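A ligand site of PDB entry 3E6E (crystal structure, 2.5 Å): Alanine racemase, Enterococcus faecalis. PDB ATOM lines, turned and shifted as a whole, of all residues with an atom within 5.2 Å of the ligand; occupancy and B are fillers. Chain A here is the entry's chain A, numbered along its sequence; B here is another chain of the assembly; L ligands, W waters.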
ATOM      1  N   VAL A  38     -11.721 -22.286  -5.190  1.00  0.00           N
ATOM      2  CA  VAL A  38     -11.510 -20.857  -5.078  1.00  0.00           C
ATOM      3  C   VAL A  38     -12.504 -20.211  -6.047  1.00  0.00           C
ATOM      4  O   VAL A  38     -12.479 -20.506  -7.244  1.00  0.00           O
ATOM      5  CB  VAL A  38     -10.055 -20.478  -5.437  1.00  0.00           C
ATOM      6  CG1 VAL A  38      -9.526 -21.398  -6.493  1.00  0.00           C
ATOM      7  CG2 VAL A  38      -9.976 -19.041  -5.905  1.00  0.00           C
ATOM      8  N   LYS A  40     -13.204 -16.591  -6.045  1.00  0.00           N
ATOM      9  CA  LYS A  40     -13.097 -15.143  -5.913  1.00  0.00           C
ATOM     10  C   LYS A  40     -13.395 -14.444  -7.234  1.00  0.00           C
ATOM     11  O   LYS A  40     -13.662 -15.106  -8.252  1.00  0.00           O
ATOM     12  CB  LYS A  40     -11.690 -14.745  -5.453  1.00  0.00           C
ATOM     13  CG  LYS A  40     -10.537 -15.294  -6.286  1.00  0.00           C
ATOM     14  CD  LYS A  40      -9.239 -14.834  -5.647  1.00  0.00           C
ATOM     15  CE  LYS A  40      -8.016 -15.469  -6.278  1.00  0.00           C
ATOM     16  NZ  LYS A  40      -7.631 -14.811  -7.545  1.00  0.00           N
ATOM     17  N   TYR A  44     -14.730 -15.887 -10.810  1.00  0.00           N
ATOM     18  CA  TYR A  44     -13.910 -15.748 -11.996  1.00  0.00           C
ATOM     19  C   TYR A  44     -14.761 -15.244 -13.138  1.00  0.00           C
ATOM     20  O   TYR A  44     -14.520 -15.567 -14.312  1.00  0.00           O
ATOM     21  CB  TYR A  44     -13.307 -17.096 -12.376  1.00  0.00           C
ATOM     22  CG  TYR A  44     -11.997 -17.426 -11.684  1.00  0.00           C
ATOM     23  CD1 TYR A  44     -11.768 -17.060 -10.356  1.00  0.00           C
ATOM     24  CD2 TYR A  44     -11.007 -18.154 -12.346  1.00  0.00           C
ATOM     25  CE1 TYR A  44     -10.576 -17.402  -9.715  1.00  0.00           C
ATOM     26  CE2 TYR A  44      -9.828 -18.495 -11.711  1.00  0.00           C
ATOM     27  CZ  TYR A  44      -9.606 -18.121 -10.400  1.00  0.00           C
ATOM     28  OH  TYR A  44      -8.447 -18.498  -9.775  1.00  0.00           O
ATOM     29  N   LEU A  86      -7.686 -16.039   1.244  1.00  0.00           N
ATOM     30  CA  LEU A  86      -6.308 -16.196   0.772  1.00  0.00           C
ATOM     31  C   LEU A  86      -5.330 -15.057   0.999  1.00  0.00           C
ATOM     32  O   LEU A  86      -4.127 -15.274   0.924  1.00  0.00           O
ATOM     33  CB  LEU A  86      -6.315 -16.522  -0.730  1.00  0.00           C
ATOM     34  CG  LEU A  86      -6.921 -17.868  -1.120  1.00  0.00           C
ATOM     35  CD1 LEU A  86      -6.991 -17.971  -2.635  1.00  0.00           C
ATOM     36  CD2 LEU A  86      -6.085 -18.984  -0.511  1.00  0.00           C
ATOM     37  N   LYS A 132       0.782 -18.543   5.712  1.00  0.00           N
ATOM     38  CA  LYS A 132       1.357 -18.610   4.380  1.00  0.00           C
ATOM     39  C   LYS A 132       2.850 -18.287   4.387  1.00  0.00           C
ATOM     40  O   LYS A 132       3.281 -17.243   4.867  1.00  0.00           O
ATOM     41  CB  LYS A 132       0.651 -17.656   3.397  1.00  0.00           C
ATOM     42  CG  LYS A 132       1.096 -17.905   1.931  1.00  0.00           C
ATOM     43  CD  LYS A 132       0.625 -16.836   0.929  1.00  0.00           C
ATOM     44  CE  LYS A 132       1.163 -17.126  -0.491  1.00  0.00           C
ATOM     45  NZ  LYS A 132       0.802 -16.090  -1.510  1.00  0.00           N
ATOM     46  N   ARG A 139       4.846 -12.448  -3.140  1.00  0.00           N
ATOM     47  CA  ARG A 139       3.739 -11.529  -2.897  1.00  0.00           C
ATOM     48  C   ARG A 139       3.473 -11.373  -1.400  1.00  0.00           C
ATOM     49  O   ARG A 139       3.437 -10.256  -0.895  1.00  0.00           O
ATOM     50  CB  ARG A 139       2.475 -12.010  -3.622  1.00  0.00           C
ATOM     51  CG  ARG A 139       2.082 -13.410  -3.251  1.00  0.00           C
ATOM     52  CD  ARG A 139       0.582 -13.561  -3.262  1.00  0.00           C
ATOM     53  NE  ARG A 139       0.035 -13.384  -4.601  1.00  0.00           N
ATOM     54  CZ  ARG A 139      -0.885 -14.202  -5.110  1.00  0.00           C
ATOM     55  NH1 ARG A 139      -1.341 -15.214  -4.384  1.00  0.00           N
ATOM     56  NH2 ARG A 139      -1.342 -13.997  -6.340  1.00  0.00           N
ATOM     57  N   PHE A 167       0.530 -23.372   4.015  1.00  0.00           N
ATOM     58  CA  PHE A 167       0.472 -23.493   2.571  1.00  0.00           C
ATOM     59  C   PHE A 167       1.349 -22.440   1.924  1.00  0.00           C
ATOM     60  O   PHE A 167       1.766 -21.459   2.570  1.00  0.00           O
ATOM     61  CB  PHE A 167      -0.957 -23.300   2.078  1.00  0.00           C
ATOM     62  CG  PHE A 167      -1.448 -21.900   2.217  1.00  0.00           C
ATOM     63  CD1 PHE A 167      -1.595 -21.082   1.098  1.00  0.00           C
ATOM     64  CD2 PHE A 167      -1.733 -21.380   3.465  1.00  0.00           C
ATOM     65  CE1 PHE A 167      -2.022 -19.758   1.231  1.00  0.00           C
ATOM     66  CE2 PHE A 167      -2.153 -20.064   3.613  1.00  0.00           C
ATOM     67  CZ  PHE A 167      -2.310 -19.250   2.497  1.00  0.00           C
ATOM     68  N   HIS A 169       2.269 -20.860  -2.430  1.00  0.00           N
ATOM     69  CA  HIS A 169       1.684 -20.768  -3.749  1.00  0.00           C
ATOM     70  C   HIS A 169       2.782 -20.768  -4.791  1.00  0.00           C
ATOM     71  O   HIS A 169       3.800 -20.107  -4.639  1.00  0.00           O
ATOM     72  CB  HIS A 169       0.847 -19.482  -3.844  1.00  0.00           C
ATOM     73  CG  HIS A 169       0.076 -19.372  -5.119  1.00  0.00           C
ATOM     74  ND1 HIS A 169      -0.927 -20.259  -5.482  1.00  0.00           N
ATOM     75  CD2 HIS A 169       0.190 -18.499  -6.154  1.00  0.00           C
ATOM     76  CE1 HIS A 169      -1.380 -19.940  -6.679  1.00  0.00           C
ATOM     77  NE2 HIS A 169      -0.723 -18.883  -7.105  1.00  0.00           N
ATOM     78  N   ASN A 206      -2.329 -25.888  -6.945  1.00  0.00           N
ATOM     79  CA  ASN A 206      -3.312 -25.079  -7.651  1.00  0.00           C
ATOM     80  C   ASN A 206      -3.693 -25.836  -8.911  1.00  0.00           C
ATOM     81  O   ASN A 206      -3.180 -26.946  -9.150  1.00  0.00           O
ATOM     82  CB  ASN A 206      -2.773 -23.679  -8.015  1.00  0.00           C
ATOM     83  CG  ASN A 206      -1.634 -23.710  -9.031  1.00  0.00           C
ATOM     84  OD1 ASN A 206      -1.079 -22.658  -9.378  1.00  0.00           O
ATOM     85  ND2 ASN A 206      -1.285 -24.896  -9.504  1.00  0.00           N
ATOM     86  N   SER A 207      -4.603 -25.263  -9.639  1.00  0.00           N
ATOM     87  CA  SER A 207      -4.950 -25.768 -10.915  1.00  0.00           C
ATOM     88  C   SER A 207      -3.799 -26.387 -11.639  1.00  0.00           C
ATOM     89  O   SER A 207      -3.783 -27.536 -11.898  1.00  0.00           O
ATOM     90  CB  SER A 207      -5.609 -24.667 -11.708  1.00  0.00           C
ATOM     91  OG  SER A 207      -6.946 -24.648 -11.459  1.00  0.00           O
ATOM     92  N   ALA A 208      -2.856 -25.566 -11.976  1.00  0.00           N
ATOM     93  CA  ALA A 208      -1.662 -26.003 -12.660  1.00  0.00           C
ATOM     94  C   ALA A 208      -0.935 -27.146 -11.944  1.00  0.00           C
ATOM     95  O   ALA A 208      -0.800 -28.238 -12.504  1.00  0.00           O
ATOM     96  CB  ALA A 208      -0.704 -24.817 -12.836  1.00  0.00           C
ATOM     97  N   ARG A 222      -6.046 -26.141  -3.910  1.00  0.00           N
ATOM     98  CA  ARG A 222      -6.899 -24.980  -4.161  1.00  0.00           C
ATOM     99  C   ARG A 222      -7.229 -24.874  -5.657  1.00  0.00           C
ATOM    100  O   ARG A 222      -6.650 -24.075  -6.378  1.00  0.00           O
ATOM    101  CB  ARG A 222      -6.182 -23.721  -3.683  1.00  0.00           C
ATOM    102  CG  ARG A 222      -6.235 -23.487  -2.178  1.00  0.00           C
ATOM    103  CD  ARG A 222      -4.846 -23.385  -1.610  1.00  0.00           C
ATOM    104  NE  ARG A 222      -3.966 -22.664  -2.517  1.00  0.00           N
ATOM    105  CZ  ARG A 222      -2.653 -22.541  -2.353  1.00  0.00           C
ATOM    106  NH1 ARG A 222      -2.061 -23.108  -1.299  1.00  0.00           N
ATOM    107  NH2 ARG A 222      -1.914 -21.901  -3.253  1.00  0.00           N
ATOM    108  N   TYR A 223      -8.171 -25.688  -6.105  1.00  0.00           N
ATOM    109  CA  TYR A 223      -8.575 -25.731  -7.514  1.00  0.00           C
ATOM    110  C   TYR A 223      -9.312 -24.481  -8.024  1.00  0.00           C
ATOM    111  O   TYR A 223     -10.424 -24.182  -7.582  1.00  0.00           O
ATOM    112  CB  TYR A 223      -9.448 -26.968  -7.754  1.00  0.00           C
ATOM    113  CG  TYR A 223      -9.177 -27.670  -9.066  1.00  0.00           C
ATOM    114  CD1 TYR A 223     -10.185 -28.377  -9.708  1.00  0.00           C
ATOM    115  CD2 TYR A 223      -7.907 -27.658  -9.657  1.00  0.00           C
ATOM    116  CE1 TYR A 223      -9.938 -29.060 -10.891  1.00  0.00           C
ATOM    117  CE2 TYR A 223      -7.661 -28.340 -10.839  1.00  0.00           C
ATOM    118  CZ  TYR A 223      -8.689 -29.035 -11.453  1.00  0.00           C
ATOM    119  OH  TYR A 223      -8.457 -29.729 -12.624  1.00  0.00           O
ATOM    120  N   GLY A 224      -8.699 -23.774  -8.966  1.00  0.00           N
ATOM    121  CA  GLY A 224      -9.326 -22.592  -9.512  1.00  0.00           C
ATOM    122  C   GLY A 224      -9.825 -22.665 -10.955  1.00  0.00           C
ATOM    123  O   GLY A 224     -10.867 -23.253 -11.228  1.00  0.00           O
ATOM    124  N   VAL A 225      -9.063 -22.054 -11.856  1.00  0.00           N
ATOM    125  CA  VAL A 225      -9.395 -21.990 -13.288  1.00  0.00           C
ATOM    126  C   VAL A 225      -9.829 -23.268 -13.974  1.00  0.00           C
ATOM    127  O   VAL A 225     -10.677 -23.226 -14.875  1.00  0.00           O
ATOM    128  CB  VAL A 225      -8.229 -21.424 -14.099  1.00  0.00           C
ATOM    129  CG1 VAL A 225      -8.026 -20.002 -13.734  1.00  0.00           C
ATOM    130  CG2 VAL A 225      -6.987 -22.227 -13.857  1.00  0.00           C
ATOM    131  N   TYR A 356      -7.669 -15.835 -17.827  1.00  0.00           N
ATOM    132  CA  TYR A 356      -7.990 -15.475 -16.442  1.00  0.00           C
ATOM    133  C   TYR A 356      -8.577 -14.058 -16.408  1.00  0.00           C
ATOM    134  O   TYR A 356      -9.536 -13.785 -15.672  1.00  0.00           O
ATOM    135  CB  TYR A 356      -6.744 -15.446 -15.558  1.00  0.00           C
ATOM    136  CG  TYR A 356      -6.265 -16.766 -14.995  1.00  0.00           C
ATOM    137  CD1 TYR A 356      -5.563 -17.671 -15.791  1.00  0.00           C
ATOM    138  CD2 TYR A 356      -6.417 -17.062 -13.640  1.00  0.00           C
ATOM    139  CE1 TYR A 356      -5.011 -18.834 -15.251  1.00  0.00           C
ATOM    140  CE2 TYR A 356      -5.867 -18.216 -13.094  1.00  0.00           C
ATOM    141  CZ  TYR A 356      -5.166 -19.100 -13.904  1.00  0.00           C
ATOM    142  OH  TYR A 356      -4.603 -20.231 -13.352  1.00  0.00           O
ATOM    143  N   TYR B 267       4.091 -14.472 -11.352  1.00  0.00           N
ATOM    144  CA  TYR B 267       3.930 -15.706 -12.122  1.00  0.00           C
ATOM    145  C   TYR B 267       4.989 -15.765 -13.203  1.00  0.00           C
ATOM    146  O   TYR B 267       5.390 -14.734 -13.736  1.00  0.00           O
ATOM    147  CB  TYR B 267       2.524 -15.762 -12.731  1.00  0.00           C
ATOM    148  CG  TYR B 267       1.457 -15.996 -11.692  1.00  0.00           C
ATOM    149  CD1 TYR B 267       1.378 -17.216 -11.013  1.00  0.00           C
ATOM    150  CD2 TYR B 267       0.590 -14.973 -11.319  1.00  0.00           C
ATOM    151  CE1 TYR B 267       0.465 -17.406  -9.994  1.00  0.00           C
ATOM    152  CE2 TYR B 267      -0.330 -15.163 -10.285  1.00  0.00           C
ATOM    153  CZ  TYR B 267      -0.378 -16.368  -9.635  1.00  0.00           C
ATOM    154  OH  TYR B 267      -1.268 -16.551  -8.599  1.00  0.00           O
ATOM    155  N   TYR B 286      -6.133  -7.389 -11.609  1.00  0.00           N
ATOM    156  CA  TYR B 286      -6.748  -7.128 -12.899  1.00  0.00           C
ATOM    157  C   TYR B 286      -8.231  -7.428 -12.862  1.00  0.00           C
ATOM    158  O   TYR B 286      -8.950  -7.063 -13.772  1.00  0.00           O
ATOM    159  CB  TYR B 286      -6.078  -7.937 -14.007  1.00  0.00           C
ATOM    160  CG  TYR B 286      -5.919  -9.414 -13.737  1.00  0.00           C
ATOM    161  CD1 TYR B 286      -7.009 -10.265 -13.776  1.00  0.00           C
ATOM    162  CD2 TYR B 286      -4.660  -9.972 -13.507  1.00  0.00           C
ATOM    163  CE1 TYR B 286      -6.864 -11.649 -13.596  1.00  0.00           C
ATOM    164  CE2 TYR B 286      -4.493 -11.353 -13.323  1.00  0.00           C
ATOM    165  CZ  TYR B 286      -5.605 -12.187 -13.379  1.00  0.00           C
ATOM    166  OH  TYR B 286      -5.485 -13.546 -13.212  1.00  0.00           O
ATOM    167  N   CYS B 313      -1.414  -9.733 -10.485  1.00  0.00           N
ATOM    168  CA  CYS B 313      -2.283 -10.867 -10.163  1.00  0.00           C
ATOM    169  C   CYS B 313      -3.755 -10.490 -10.297  1.00  0.00           C
ATOM    170  O   CYS B 313      -4.108  -9.346 -10.572  1.00  0.00           O
ATOM    171  CB  CYS B 313      -2.059 -11.357  -8.724  1.00  0.00           C
ATOM    172  SG  CYS B 313      -0.343 -11.751  -8.269  1.00  0.00           S
ATOM    173  N   MET B 314      -4.629 -11.459 -10.081  1.00  0.00           N
ATOM    174  CA  MET B 314      -6.051 -11.220 -10.152  1.00  0.00           C
ATOM    175  C   MET B 314      -6.446 -10.249  -9.044  1.00  0.00           C
ATOM    176  O   MET B 314      -7.197  -9.303  -9.295  1.00  0.00           O
ATOM    177  CB  MET B 314      -6.806 -12.531  -9.998  1.00  0.00           C
ATOM    178  CG  MET B 314      -8.275 -12.437 -10.356  1.00  0.00           C
ATOM    179  SD  MET B 314      -9.125 -13.992 -10.093  1.00  0.00           S
ATOM    180  CE  MET B 314      -8.531 -14.937 -11.458  1.00  0.00           C
ATOM    181  N   ASP B 315      -5.919 -10.452  -7.843  1.00  0.00           N
ATOM    182  CA  ASP B 315      -6.279  -9.601  -6.704  1.00  0.00           C
ATOM    183  C   ASP B 315      -5.208  -8.720  -6.096  1.00  0.00           C
ATOM    184  O   ASP B 315      -5.479  -8.009  -5.118  1.00  0.00           O
ATOM    185  CB  ASP B 315      -6.889 -10.469  -5.605  1.00  0.00           C
ATOM    186  CG  ASP B 315      -8.147 -11.137  -6.055  1.00  0.00           C
ATOM    187  OD1 ASP B 315      -9.170 -10.425  -6.176  1.00  0.00           O
ATOM    188  OD2 ASP B 315      -8.114 -12.360  -6.324  1.00  0.00           O
ATOM    189  N   GLN B 316      -4.008  -8.755  -6.643  1.00  0.00           N
ATOM    190  CA  GLN B 316      -2.953  -7.909  -6.119  1.00  0.00           C
ATOM    191  C   GLN B 316      -1.743  -7.817  -7.029  1.00  0.00           C
ATOM    192  O   GLN B 316      -1.647  -8.542  -8.022  1.00  0.00           O
ATOM    193  CB  GLN B 316      -2.534  -8.381  -4.721  1.00  0.00           C
ATOM    194  CG  GLN B 316      -2.300  -9.870  -4.587  1.00  0.00           C
ATOM    195  CD  GLN B 316      -3.318 -10.528  -3.683  1.00  0.00           C
ATOM    196  OE1 GLN B 316      -4.428 -10.847  -4.101  1.00  0.00           O
ATOM    197  NE2 GLN B 316      -2.935 -10.719  -2.412  1.00  0.00           N
HETATM  198  N1  LIG L   1      -4.268 -20.303  -4.310  1.00  0.00           N
HETATM  199  C1  LIG L   1      -3.880 -18.934  -4.162  1.00  0.00           C
HETATM  200  C2  LIG L   1      -3.104 -18.456  -2.944  1.00  0.00           C
HETATM  201  C3  LIG L   1      -4.235 -18.049  -5.190  1.00  0.00           C
HETATM  202  O1  LIG L   1      -3.909 -16.738  -5.130  1.00  0.00           O
HETATM  203  C4  LIG L   1      -4.972 -18.555  -6.330  1.00  0.00           C
HETATM  204  C5  LIG L   1      -5.358 -17.618  -7.451  1.00  0.00           C
HETATM  205  C6  LIG L   1      -5.314 -19.984  -6.384  1.00  0.00           C
HETATM  206  C7  LIG L   1      -4.956 -20.807  -5.374  1.00  0.00           C
HETATM  207  C8  LIG L   1      -6.071 -20.603  -7.528  1.00  0.00           C
HETATM  208  O2  LIG L   1      -5.249 -20.563  -8.693  1.00  0.00           O
HETATM  209  P1  LIG L   1      -5.652 -21.125 -10.132  1.00  0.00           P
HETATM  210  O3  LIG L   1      -5.886 -22.541  -9.972  1.00  0.00           O
HETATM  211  O4  LIG L   1      -6.848 -20.414 -10.590  1.00  0.00           O
HETATM  212  O5  LIG L   1      -4.536 -20.882 -11.031  1.00  0.00           O
HETATM  213  N2  LIG L   1      -4.117 -16.956  -8.039  1.00  0.00           N
HETATM  214  C9  LIG L   1      -4.213 -16.043  -9.094  1.00  0.00           C
HETATM  215  C10 LIG L   1      -4.085 -14.627  -8.977  1.00  0.00           C
HETATM  216  O6  LIG L   1      -3.872 -13.940  -7.813  1.00  0.00           O
HETATM  217  N3  LIG L   1      -4.194 -14.096 -10.166  1.00  0.00           N
HETATM  218  O7  LIG L   1      -4.401 -15.114 -11.082  1.00  0.00           O
HETATM  219  C11 LIG L   1      -4.414 -16.291 -10.421  1.00  0.00           C
HETATM  220  O   HOH W   1      -2.882 -23.057 -11.933  1.00  0.00           O
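The side-chain sulfur (SD) of Met 314 of chain B sits at hydrogen-bond distance from the side-chain amino group (NZ) of Lys 40 (3.1 Å). OG of Ser 207 is in hydrogen-bond range of N of Val 225 (3.4 Å). N of Tyr 286 of chain B lies within hydrogen-bond range of O of Cys 313 of chain B, 3.0 Å away. The side-chain hydroxyl of Tyr 267 of chain B lies within hydrogen-bond range of the guanidinium group of Arg 139, at 3.4 Å. NH2 of Arg 139 lies within hydrogen-bond range of SG of Cys 313 of chain B. A ring nitrogen (NE2) of His 169 lies within hydrogen-bond range of the side-chain hydroxyl (OH) of Tyr 267 of chain B, 2.8 Å away. The guanidinium group (NH2) of Arg 222 lies within hydrogen-bond range of a ring nitrogen (ND1) of His 169 (2.9 Å). The backbone carbonyl oxygen of Gln 316 of chain B lies close to the side-chain sulfur of Cys 313 of chain B (3.5 Å).
Water W1 lies within hydrogen-bond range of N of Ala 208 (2.5 Å), O5 of the ligand (2.9 Å) and OD1 of Asn 206 (3.2 Å).
The side-chain hydroxyl of Tyr 356 is in hydrogen-bond range of an oxygen (O5) of the ligand, 2.4 Å away. The side-chain hydroxyl (OH) of Tyr 44 sits at hydrogen-bond distance from an oxygen (O4) of the ligand, 2.6 Å away. The backbone NH of Met 314 of chain B lies close to an oxygen (O6) of the ligand, at 3.4 Å. N of Ser 207 sits close to O3 of the ligand, at 3.0 Å. OG of Ser 207 lies close to O3 of the ligand, at 2.8 Å. O7 of the ligand sits at hydrogen-bond distance from OH of Tyr 286 of chain B. O6 of the ligand sits at hydrogen-bond distance from NH2 of Arg 139 (2.9 Å). OH of Tyr 267 of chain B is in hydrogen-bond range of N2 of the ligand (2.9 Å). A nitrogen (N1) of the ligand sits at hydrogen-bond distance from the guanidinium group (NE) of Arg 222 (3.0 Å). The backbone NH (N) of Val 225 sits at hydrogen-bond distance from an oxygen (O4) of the ligand (3.0 Å). O3 of the ligand lies within hydrogen-bond range of N of Gly 224 (3.2 Å).
Val 38 touches the ligand. Lys 40 touches the ligand (NZ to C5, 3.6 Å). Leu 86 touches the ligand (CD1 to C1, 3.6 Å). His 169 touches the ligand. Asn 206 touches the ligand. Cys 313 of chain B touches the ligand. Hydrophobic or aromatic side chains that line the ligand: Val 38, Tyr 44, Leu 86, His 169, Val 225, Tyr 356, Tyr 267 of chain B, Tyr 286 of chain B and Met 314 of chain B.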
